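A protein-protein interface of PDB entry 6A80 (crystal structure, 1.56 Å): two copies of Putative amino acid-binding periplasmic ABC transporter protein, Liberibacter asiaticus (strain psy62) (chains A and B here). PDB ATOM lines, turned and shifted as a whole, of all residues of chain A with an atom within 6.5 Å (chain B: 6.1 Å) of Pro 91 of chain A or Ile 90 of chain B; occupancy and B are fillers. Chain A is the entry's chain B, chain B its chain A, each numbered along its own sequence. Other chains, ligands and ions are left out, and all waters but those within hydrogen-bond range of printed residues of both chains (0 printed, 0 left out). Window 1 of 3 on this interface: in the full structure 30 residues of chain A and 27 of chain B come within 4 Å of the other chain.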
ATOM      1  N   ILE A  78       5.973  19.514   5.217  1.00  0.00           N
ATOM      2  CA  ILE A  78       5.719  20.406   6.357  1.00  0.00           C
ATOM      3  C   ILE A  78       7.006  20.935   6.917  1.00  0.00           C
ATOM      4  O   ILE A  78       7.967  20.190   7.147  1.00  0.00           O
ATOM      5  CB  ILE A  78       4.950  19.617   7.421  1.00  0.00           C
ATOM      6  CG1 ILE A  78       3.615  19.151   6.818  1.00  0.00           C
ATOM      7  CG2 ILE A  78       4.730  20.466   8.701  1.00  0.00           C
ATOM      8  CD1 ILE A  78       2.691  18.362   7.803  1.00  0.00           C
ATOM      9  N   GLN A  83       4.269  26.136   8.566  1.00  0.00           N
ATOM     10  CA  GLN A  83       3.182  25.973   9.529  1.00  0.00           C
ATOM     11  C   GLN A  83       2.784  27.319  10.157  1.00  0.00           C
ATOM     12  O   GLN A  83       1.660  27.481  10.595  1.00  0.00           O
ATOM     13  CB  GLN A  83       3.541  24.972  10.641  1.00  0.00           C
ATOM     14  CG  GLN A  83       3.416  23.519  10.185  1.00  0.00           C
ATOM     15  CD  GLN A  83       4.009  22.593  11.234  1.00  0.00           C
ATOM     16  OE1 GLN A  83       5.095  22.846  11.716  1.00  0.00           O
ATOM     17  NE2 GLN A  83       3.264  21.594  11.647  1.00  0.00           N
ATOM     18  N   SER A  89      -3.124  20.063   5.891  1.00  0.00           N
ATOM     19  CA  SER A  89      -3.891  18.906   6.262  1.00  0.00           C
ATOM     20  C   SER A  89      -3.014  18.025   7.165  1.00  0.00           C
ATOM     21  O   SER A  89      -1.793  18.252   7.382  1.00  0.00           O
ATOM     22  CB  SER A  89      -4.287  18.084   5.022  1.00  0.00           C
ATOM     23  OG  SER A  89      -3.104  17.443   4.501  1.00  0.00           O
ATOM     24  N   ILE A  90      -3.694  17.042   7.738  1.00  0.00           N
ATOM     25  CA  ILE A  90      -2.955  15.926   8.386  1.00  0.00           C
ATOM     26  C   ILE A  90      -1.981  15.341   7.322  1.00  0.00           C
ATOM     27  O   ILE A  90      -2.351  15.307   6.136  1.00  0.00           O
ATOM     28  CB  ILE A  90      -3.978  14.857   8.839  1.00  0.00           C
ATOM     29  CG1 ILE A  90      -3.305  13.768   9.720  1.00  0.00           C
ATOM     30  CG2 ILE A  90      -4.695  14.144   7.677  1.00  0.00           C
ATOM     31  CD1 ILE A  90      -4.365  12.860  10.371  1.00  0.00           C
ATOM     32  N   PRO A  91      -0.835  14.783   7.760  1.00  0.00           N
ATOM     33  CA  PRO A  91       0.085  14.222   6.738  1.00  0.00           C
ATOM     34  C   PRO A  91      -0.550  13.038   6.083  1.00  0.00           C
ATOM     35  O   PRO A  91      -1.263  12.276   6.732  1.00  0.00           O
ATOM     36  CB  PRO A  91       1.327  13.832   7.565  1.00  0.00           C
ATOM     37  CG  PRO A  91       1.294  14.781   8.742  1.00  0.00           C
ATOM     38  CD  PRO A  91      -0.173  14.885   9.075  1.00  0.00           C
ATOM     39  N   TYR A  92      -0.232  12.842   4.800  1.00  0.00           N
ATOM     40  CA  TYR A  92      -0.761  11.667   4.044  1.00  0.00           C
ATOM     41  C   TYR A  92       0.289  10.772   3.421  1.00  0.00           C
ATOM     42  O   TYR A  92      -0.061   9.658   2.963  1.00  0.00           O
ATOM     43  CB  TYR A  92      -1.817  12.086   2.980  1.00  0.00           C
ATOM     44  CG  TYR A  92      -1.270  12.908   1.840  1.00  0.00           C
ATOM     45  CD1 TYR A  92      -0.600  12.292   0.786  1.00  0.00           C
ATOM     46  CD2 TYR A  92      -1.518  14.276   1.790  1.00  0.00           C
ATOM     47  CE1 TYR A  92      -0.110  13.064  -0.274  1.00  0.00           C
ATOM     48  CE2 TYR A  92      -1.052  15.064   0.753  1.00  0.00           C
ATOM     49  CZ  TYR A  92      -0.401  14.456  -0.299  1.00  0.00           C
ATOM     50  OH  TYR A  92       0.047  15.197  -1.356  1.00  0.00           O
ATOM     51  N   ILE A  93       1.532  11.210   3.541  1.00  0.00           N
ATOM     52  CA  ILE A  93       2.693  10.395   3.071  1.00  0.00           C
ATOM     53  C   ILE A  93       3.937  10.955   3.685  1.00  0.00           C
ATOM     54  O   ILE A  93       3.943  12.025   4.338  1.00  0.00           O
ATOM     55  CB  ILE A  93       2.755  10.291   1.509  1.00  0.00           C
ATOM     56  CG1 ILE A  93       3.734   9.130   1.108  1.00  0.00           C
ATOM     57  CG2 ILE A  93       3.208  11.608   0.899  1.00  0.00           C
ATOM     58  CD1 ILE A  93       3.295   8.476  -0.187  1.00  0.00           C
ATOM     59  N   ALA A 191       7.278  14.512   6.892  1.00  0.00           N
ATOM     60  CA  ALA A 191       5.882  14.513   6.649  1.00  0.00           C
ATOM     61  C   ALA A 191       5.452  15.419   5.487  1.00  0.00           C
ATOM     62  O   ALA A 191       5.998  16.507   5.311  1.00  0.00           O
ATOM     63  CB  ALA A 191       5.154  15.011   7.912  1.00  0.00           C
ATOM     64  N   VAL A 192       4.524  14.876   4.694  1.00  0.00           N
ATOM     65  CA  VAL A 192       4.091  15.563   3.471  1.00  0.00           C
ATOM     66  C   VAL A 192       2.579  15.706   3.584  1.00  0.00           C
ATOM     67  O   VAL A 192       1.822  14.756   4.007  1.00  0.00           O
ATOM     68  CB  VAL A 192       4.539  14.782   2.212  1.00  0.00           C
ATOM     69  CG1 VAL A 192       3.761  15.300   0.983  1.00  0.00           C
ATOM     70  CG2 VAL A 192       6.026  14.920   2.067  1.00  0.00           C
ATOM     71  N   ALA A 193       2.063  16.915   3.252  1.00  0.00           N
ATOM     72  CA  ALA A 193       0.611  17.165   3.407  1.00  0.00           C
ATOM     73  C   ALA A 193       0.070  18.083   2.303  1.00  0.00           C
ATOM     74  O   ALA A 193       0.859  18.538   1.426  1.00  0.00           O
ATOM     75  CB  ALA A 193       0.319  17.796   4.822  1.00  0.00           C
ATOM     76  N   PHE A 194      -1.266  18.259   2.306  1.00  0.00           N
ATOM     77  CA  PHE A 194      -1.870  19.318   1.432  1.00  0.00           C
ATOM     78  C   PHE A 194      -1.671  20.648   2.146  1.00  0.00           C
ATOM     79  O   PHE A 194      -1.745  20.719   3.371  1.00  0.00           O
ATOM     80  CB  PHE A 194      -3.343  19.072   1.197  1.00  0.00           C
ATOM     81  CG  PHE A 194      -3.605  17.802   0.425  1.00  0.00           C
ATOM     82  CD1 PHE A 194      -3.227  17.694  -0.916  1.00  0.00           C
ATOM     83  CD2 PHE A 194      -4.243  16.727   1.042  1.00  0.00           C
ATOM     84  CE1 PHE A 194      -3.448  16.510  -1.652  1.00  0.00           C
ATOM     85  CE2 PHE A 194      -4.524  15.574   0.315  1.00  0.00           C
ATOM     86  CZ  PHE A 194      -4.091  15.448  -1.028  1.00  0.00           C
ATOM     87  N   ASN A 208      -9.299  16.728   6.090  1.00  0.00           N
ATOM     88  CA  ASN A 208      -8.906  15.786   7.133  1.00  0.00           C
ATOM     89  C   ASN A 208      -9.925  14.683   7.351  1.00  0.00           C
ATOM     90  O   ASN A 208      -9.553  13.486   7.407  1.00  0.00           O
ATOM     91  CB  ASN A 208      -8.517  16.474   8.448  1.00  0.00           C
ATOM     92  CG  ASN A 208      -7.303  17.307   8.321  1.00  0.00           C
ATOM     93  OD1 ASN A 208      -6.547  17.180   7.322  1.00  0.00           O
ATOM     94  ND2 ASN A 208      -7.060  18.167   9.295  1.00  0.00           N
ATOM     95  N   LEU A 211      -9.713  12.368   4.373  1.00  0.00           N
ATOM     96  CA  LEU A 211      -8.454  11.525   4.444  1.00  0.00           C
ATOM     97  C   LEU A 211      -8.603  10.348   5.432  1.00  0.00           C
ATOM     98  O   LEU A 211      -8.199   9.202   5.119  1.00  0.00           O
ATOM     99  CB  LEU A 211      -7.204  12.336   4.783  1.00  0.00           C
ATOM    100  CG  LEU A 211      -6.700  13.186   3.555  1.00  0.00           C
ATOM    101  CD1 LEU A 211      -5.621  14.095   4.046  1.00  0.00           C
ATOM    102  CD2 LEU A 211      -6.278  12.335   2.325  1.00  0.00           C
ATOM    103  N   HIS A 215      -8.531   6.357   4.476  1.00  0.00           N
ATOM    104  CA  HIS A 215      -7.603   5.430   5.189  1.00  0.00           C
ATOM    105  C   HIS A 215      -8.491   4.222   5.626  1.00  0.00           C
ATOM    106  O   HIS A 215      -8.078   3.072   5.515  1.00  0.00           O
ATOM    107  CB  HIS A 215      -6.933   5.989   6.493  1.00  0.00           C
ATOM    108  CG  HIS A 215      -5.587   6.689   6.292  1.00  0.00           C
ATOM    109  ND1 HIS A 215      -4.393   6.004   6.161  1.00  0.00           N
ATOM    110  CD2 HIS A 215      -5.254   8.013   6.247  1.00  0.00           C
ATOM    111  CE1 HIS A 215      -3.390   6.859   6.018  1.00  0.00           C
ATOM    112  NE2 HIS A 215      -3.886   8.086   6.047  1.00  0.00           N
ATOM    113  N   VAL A 236       1.973   6.817   6.369  1.00  0.00           N
ATOM    114  CA  VAL A 236       1.826   7.534   7.643  1.00  0.00           C
ATOM    115  C   VAL A 236       0.719   6.804   8.412  1.00  0.00           C
ATOM    116  O   VAL A 236      -0.031   6.053   7.777  1.00  0.00           O
ATOM    117  CB  VAL A 236       1.321   8.943   7.414  1.00  0.00           C
ATOM    118  CG1 VAL A 236       2.491   9.769   6.821  1.00  0.00           C
ATOM    119  CG2 VAL A 236       0.075   8.978   6.544  1.00  0.00           C
ATOM    120  N   PRO A 237       0.618   7.032   9.720  1.00  0.00           N
ATOM    121  CA  PRO A 237      -0.395   6.237  10.404  1.00  0.00           C
ATOM    122  C   PRO A 237      -1.796   6.375   9.908  1.00  0.00           C
ATOM    123  O   PRO A 237      -2.154   7.448   9.495  1.00  0.00           O
ATOM    124  CB  PRO A 237      -0.367   6.729  11.875  1.00  0.00           C
ATOM    125  CG  PRO A 237       0.672   7.793  12.002  1.00  0.00           C
ATOM    126  CD  PRO A 237       1.393   7.929  10.629  1.00  0.00           C
ATOM    127  N   ILE B  78      -7.135   9.801  16.744  1.00  0.00           N
ATOM    128  CA  ILE B  78      -7.988  10.489  15.771  1.00  0.00           C
ATOM    129  C   ILE B  78      -9.012   9.510  15.225  1.00  0.00           C
ATOM    130  O   ILE B  78      -8.675   8.401  14.754  1.00  0.00           O
ATOM    131  CB  ILE B  78      -7.105  11.048  14.628  1.00  0.00           C
ATOM    132  CG1 ILE B  78      -6.104  12.069  15.244  1.00  0.00           C
ATOM    133  CG2 ILE B  78      -7.977  11.814  13.642  1.00  0.00           C
ATOM    134  CD1 ILE B  78      -5.151  12.743  14.238  1.00  0.00           C
ATOM    135  N   PHE B  88      -7.598  18.694  16.192  1.00  0.00           N
ATOM    136  CA  PHE B  88      -6.423  17.901  16.626  1.00  0.00           C
ATOM    137  C   PHE B  88      -5.160  18.603  16.202  1.00  0.00           C
ATOM    138  O   PHE B  88      -5.116  19.267  15.125  1.00  0.00           O
ATOM    139  CB  PHE B  88      -6.392  16.552  15.932  1.00  0.00           C
ATOM    140  CG  PHE B  88      -7.350  15.537  16.514  1.00  0.00           C
ATOM    141  CD1 PHE B  88      -7.034  14.826  17.727  1.00  0.00           C
ATOM    142  CD2 PHE B  88      -8.544  15.228  15.877  1.00  0.00           C
ATOM    143  CE1 PHE B  88      -7.907  13.842  18.222  1.00  0.00           C
ATOM    144  CE2 PHE B  88      -9.416  14.256  16.379  1.00  0.00           C
ATOM    145  CZ  PHE B  88      -9.119  13.565  17.555  1.00  0.00           C
ATOM    146  N   SER B  89      -4.106  18.440  16.976  1.00  0.00           N
ATOM    147  CA  SER B  89      -2.739  18.677  16.501  1.00  0.00           C
ATOM    148  C   SER B  89      -2.375  17.689  15.380  1.00  0.00           C
ATOM    149  O   SER B  89      -3.076  16.728  15.122  1.00  0.00           O
ATOM    150  CB  SER B  89      -1.732  18.577  17.628  1.00  0.00           C
ATOM    151  OG  SER B  89      -1.516  17.198  18.017  1.00  0.00           O
ATOM    152  N   ILE B  90      -1.275  18.018  14.715  1.00  0.00           N
ATOM    153  CA  ILE B  90      -0.623  17.031  13.895  1.00  0.00           C
ATOM    154  C   ILE B  90      -0.371  15.769  14.770  1.00  0.00           C
ATOM    155  O   ILE B  90      -0.076  15.889  15.952  1.00  0.00           O
ATOM    156  CB  ILE B  90       0.668  17.676  13.355  1.00  0.00           C
ATOM    157  CG1 ILE B  90       1.231  16.782  12.253  1.00  0.00           C
ATOM    158  CG2 ILE B  90       1.702  17.962  14.448  1.00  0.00           C
ATOM    159  CD1 ILE B  90       2.457  17.441  11.584  1.00  0.00           C
ATOM    160  N   PRO B  91      -0.450  14.559  14.193  1.00  0.00           N
ATOM    161  CA  PRO B  91      -0.158  13.402  15.043  1.00  0.00           C
ATOM    162  C   PRO B  91       1.267  13.402  15.577  1.00  0.00           C
ATOM    163  O   PRO B  91       2.258  13.838  14.831  1.00  0.00           O
ATOM    164  CB  PRO B  91      -0.292  12.211  14.047  1.00  0.00           C
ATOM    165  CG  PRO B  91      -1.311  12.708  12.985  1.00  0.00           C
ATOM    166  CD  PRO B  91      -0.947  14.179  12.850  1.00  0.00           C
ATOM    167  N   TYR B  92       1.424  12.921  16.824  1.00  0.00           N
ATOM    168  CA  TYR B  92       2.759  12.871  17.410  1.00  0.00           C
ATOM    169  C   TYR B  92       3.224  11.486  17.794  1.00  0.00           C
ATOM    170  O   TYR B  92       4.378  11.325  18.191  1.00  0.00           O
ATOM    171  CB  TYR B  92       2.923  13.864  18.573  1.00  0.00           C
ATOM    172  CG  TYR B  92       2.033  13.548  19.783  1.00  0.00           C
ATOM    173  CD1 TYR B  92       2.447  12.568  20.700  1.00  0.00           C
ATOM    174  CD2 TYR B  92       0.874  14.224  20.012  1.00  0.00           C
ATOM    175  CE1 TYR B  92       1.677  12.281  21.824  1.00  0.00           C
ATOM    176  CE2 TYR B  92       0.081  13.994  21.147  1.00  0.00           C
ATOM    177  CZ  TYR B  92       0.479  13.003  22.039  1.00  0.00           C
ATOM    178  OH  TYR B  92      -0.297  12.805  23.185  1.00  0.00           O
ATOM    179  N   VAL B 192      -2.286   9.317  16.733  1.00  0.00           N
ATOM    180  CA  VAL B 192      -2.602   9.884  18.061  1.00  0.00           C
ATOM    181  C   VAL B 192      -2.128  11.276  18.136  1.00  0.00           C
ATOM    182  O   VAL B 192      -1.028  11.624  17.642  1.00  0.00           O
ATOM    183  CB  VAL B 192      -1.910   9.046  19.143  1.00  0.00           C
ATOM    184  CG1 VAL B 192      -2.064   9.730  20.502  1.00  0.00           C
ATOM    185  CG2 VAL B 192      -2.507   7.661  19.196  1.00  0.00           C
ATOM    186  N   ALA B 193      -2.961  12.131  18.683  1.00  0.00           N
ATOM    187  CA  ALA B 193      -2.699  13.569  18.645  1.00  0.00           C
ATOM    188  C   ALA B 193      -3.192  14.279  19.921  1.00  0.00           C
ATOM    189  O   ALA B 193      -3.868  13.648  20.765  1.00  0.00           O
ATOM    190  CB  ALA B 193      -3.343  14.206  17.393  1.00  0.00           C
ATOM    191  N   PHE B 194      -2.816  15.551  20.087  1.00  0.00           N
ATOM    192  CA  PHE B 194      -3.494  16.394  21.153  1.00  0.00           C
ATOM    193  C   PHE B 194      -4.859  16.821  20.627  1.00  0.00           C
ATOM    194  O   PHE B 194      -4.960  17.163  19.477  1.00  0.00           O
ATOM    195  CB  PHE B 194      -2.646  17.610  21.460  1.00  0.00           C
ATOM    196  CG  PHE B 194      -1.312  17.296  22.052  1.00  0.00           C
ATOM    197  CD1 PHE B 194      -1.230  16.663  23.296  1.00  0.00           C
ATOM    198  CD2 PHE B 194      -0.125  17.621  21.358  1.00  0.00           C
ATOM    199  CE1 PHE B 194       0.045  16.317  23.874  1.00  0.00           C
ATOM    200  CE2 PHE B 194       1.115  17.268  21.908  1.00  0.00           C
ATOM    201  CZ  PHE B 194       1.223  16.630  23.156  1.00  0.00           C
ATOM    202  N   THR B 204      -3.730  25.648  17.900  1.00  0.00           N
ATOM    203  CA  THR B 204      -3.427  24.385  17.146  1.00  0.00           C
ATOM    204  C   THR B 204      -2.209  24.608  16.229  1.00  0.00           C
ATOM    205  O   THR B 204      -1.236  23.821  16.299  1.00  0.00           O
ATOM    206  CB  THR B 204      -4.663  23.936  16.331  1.00  0.00           C
ATOM    207  OG1 THR B 204      -5.728  23.676  17.253  1.00  0.00           O
ATOM    208  CG2 THR B 204      -4.385  22.645  15.548  1.00  0.00           C
ATOM    209  N   ILE B 207       0.978  24.825  18.350  1.00  0.00           N
ATOM    210  CA  ILE B 207       1.426  23.533  18.885  1.00  0.00           C
ATOM    211  C   ILE B 207       2.100  22.777  17.730  1.00  0.00           C
ATOM    212  O   ILE B 207       3.163  22.137  17.965  1.00  0.00           O
ATOM    213  CB  ILE B 207       0.222  22.752  19.493  1.00  0.00           C
ATOM    214  CG1 ILE B 207      -0.274  23.423  20.812  1.00  0.00           C
ATOM    215  CG2 ILE B 207       0.519  21.251  19.697  1.00  0.00           C
ATOM    216  CD1 ILE B 207      -1.491  22.713  21.422  1.00  0.00           C
ATOM    217  N   ASN B 208       1.455  22.819  16.561  1.00  0.00           N
ATOM    218  CA  ASN B 208       2.002  22.114  15.388  1.00  0.00           C
ATOM    219  C   ASN B 208       3.395  22.580  15.037  1.00  0.00           C
ATOM    220  O   ASN B 208       4.310  21.776  14.803  1.00  0.00           O
ATOM    221  CB  ASN B 208       1.072  22.158  14.183  1.00  0.00           C
ATOM    222  CG  ASN B 208      -0.204  21.402  14.407  1.00  0.00           C
ATOM    223  OD1 ASN B 208      -0.297  20.631  15.365  1.00  0.00           O
ATOM    224  ND2 ASN B 208      -1.147  21.527  13.511  1.00  0.00           N
ATOM    225  N   LEU B 211       5.726  21.278  17.653  1.00  0.00           N
ATOM    226  CA  LEU B 211       5.998  19.837  17.484  1.00  0.00           C
ATOM    227  C   LEU B 211       7.040  19.640  16.336  1.00  0.00           C
ATOM    228  O   LEU B 211       7.967  18.836  16.529  1.00  0.00           O
ATOM    229  CB  LEU B 211       4.714  19.020  17.245  1.00  0.00           C
ATOM    230  CG  LEU B 211       3.849  18.823  18.511  1.00  0.00           C
ATOM    231  CD1 LEU B 211       2.495  18.340  18.016  1.00  0.00           C
ATOM    232  CD2 LEU B 211       4.585  17.848  19.441  1.00  0.00           C
ATOM    233  N   CYS B 212       6.925  20.360  15.211  1.00  0.00           N
ATOM    234  CA  CYS B 212       7.933  20.211  14.154  1.00  0.00           C
ATOM    235  C   CYS B 212       9.334  20.658  14.638  1.00  0.00           C
ATOM    236  O   CYS B 212      10.371  20.008  14.382  1.00  0.00           O
ATOM    237  CB  CYS B 212       7.497  20.893  12.858  1.00  0.00           C
ATOM    238  SG  CYS B 212       6.416  19.933  11.788  1.00  0.00           S
ATOM    239  N   PRO B 237       6.262  10.486  11.152  1.00  0.00           N
ATOM    240  CA  PRO B 237       7.362  11.134  10.388  1.00  0.00           C
ATOM    241  C   PRO B 237       7.869  12.346  11.039  1.00  0.00           C
ATOM    242  O   PRO B 237       7.129  12.952  11.835  1.00  0.00           O
ATOM    243  CB  PRO B 237       6.706  11.439   9.041  1.00  0.00           C
ATOM    244  CG  PRO B 237       5.261  11.341   9.258  1.00  0.00           C
ATOM    245  CD  PRO B 237       5.029  10.377  10.388  1.00  0.00           C
ATOM    246  N   CYS B 239       9.749  16.284  10.482  1.00  0.00           N
ATOM    247  CA  CYS B 239       9.442  17.456   9.668  1.00  0.00           C
ATOM    248  C   CYS B 239      10.733  17.947   9.013  1.00  0.00           C
ATOM    249  O   CYS B 239      11.816  17.396   9.235  1.00  0.00           O
ATOM    250  CB  CYS B 239       8.865  18.596  10.483  1.00  0.00           C
ATOM    251  SG  CYS B 239       7.447  18.164  11.518  1.00  0.00           S
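The side-chain amide oxygen (OD1) of Asn 208 of chain B lies within hydrogen-bond range of the backbone NH (N) of Ile 90 of chain B, at 2.9 Å.
The backbone carbonyl oxygen (O) of Thr 204 of chain B lies close to the side-chain amide oxygen (OD1) of Asn 208 of chain B (3.5 Å).
SG of Cys 212 of chain B forms a disulfide with SG of Cys 239 of chain B (2.1 Å).
The backbone NH (N) of Ile 78 of chain A sits at hydrogen-bond distance from the backbone carbonyl oxygen (O) of Ala 191 of chain A, at 3.0 Å.
N of Ile 90 of chain A lies within hydrogen-bond range of OD1 of Asn 208 of chain A (2.9 Å).
Hydrophobic or aromatic side chains of chain B within 4 Å of the printed part of chain A: Ile 78, Ile 90, Pro 91 and Pro 237.
O of Asn 208 of chain B is in hydrogen-bond range of NE2 of Gln 83 of chain A (3.3 Å).
The side-chain sulfur (SG) of Cys 212 of chain B lies close to the side-chain amide oxygen (OE1) of Gln 83 of chain A (3.2 Å).
Ile 78 of chain A touches Ile 90 of chain B, and with the chains exchanged Ile 90 of chain A touches Ile 78 of chain B.
Ile 90 of chain A touches Pro 91 of chain B, and with the chains exchanged Pro 91 of chain A touches Ile 90 of chain B.
Pro 91 of chain A touches its own counterpart, Pro 91 of chain B.
11 positions are printed for both chains.
Of the 10 pairs that touch across the chains among the printed residues, 5 have their exchanged pair printed and touching as well.
Of the printed residues of chain B, Gln 83 of chain A touches Asn 208 and Cys 212.
Of the printed residues of chain B, Ile 90 of chain A touches Ile 78 and Pro 91.
Pro 91 of chain A touches just these residues of chain B: Ile 90 (3.96 Å) and Pro 91 (3.9 Å).
Asn 208 of chain A touches none of the printed residues of chain B.
His 215 of chain A touches none of the printed residues of chain B.
Of chain A, only Ile 78 and Pro 91 come within 4 Å of Ile 90 of chain B.
Printed residues of chain A within 4 Å of Pro 237 of chain B: Ala 191.
The nearest residue of chain A that does not touch Ile 90 of chain B is Gln 83 of chain A (4.2 Å).
The nearest printed residue of chain B that does not touch Ile 90 of chain A is Ile 90 of chain B (5.8 Å).
Among the printed residues, pairs that only touch across the chains: Ile 78 of chain A with Cys 212 of chain B (3.6 Å), Ala 191 of chain A with Pro 237 of chain B (3.8 Å), Ile 78 of chain A with Cys 239 of chain B (3.8 Å), Ile 78 of chain A with Ile 90 of chain B (3.9 Å), Pro 91 of chain A with Pro 91 of chain B (3.9 Å), Ile 90 of chain A with Pro 91 of chain B (3.9 Å), Ile 90 of chain A with Ile 78 of chain B (3.9 Å) and Pro 91 of chain A with Ile 90 of chain B (3.96 Å).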
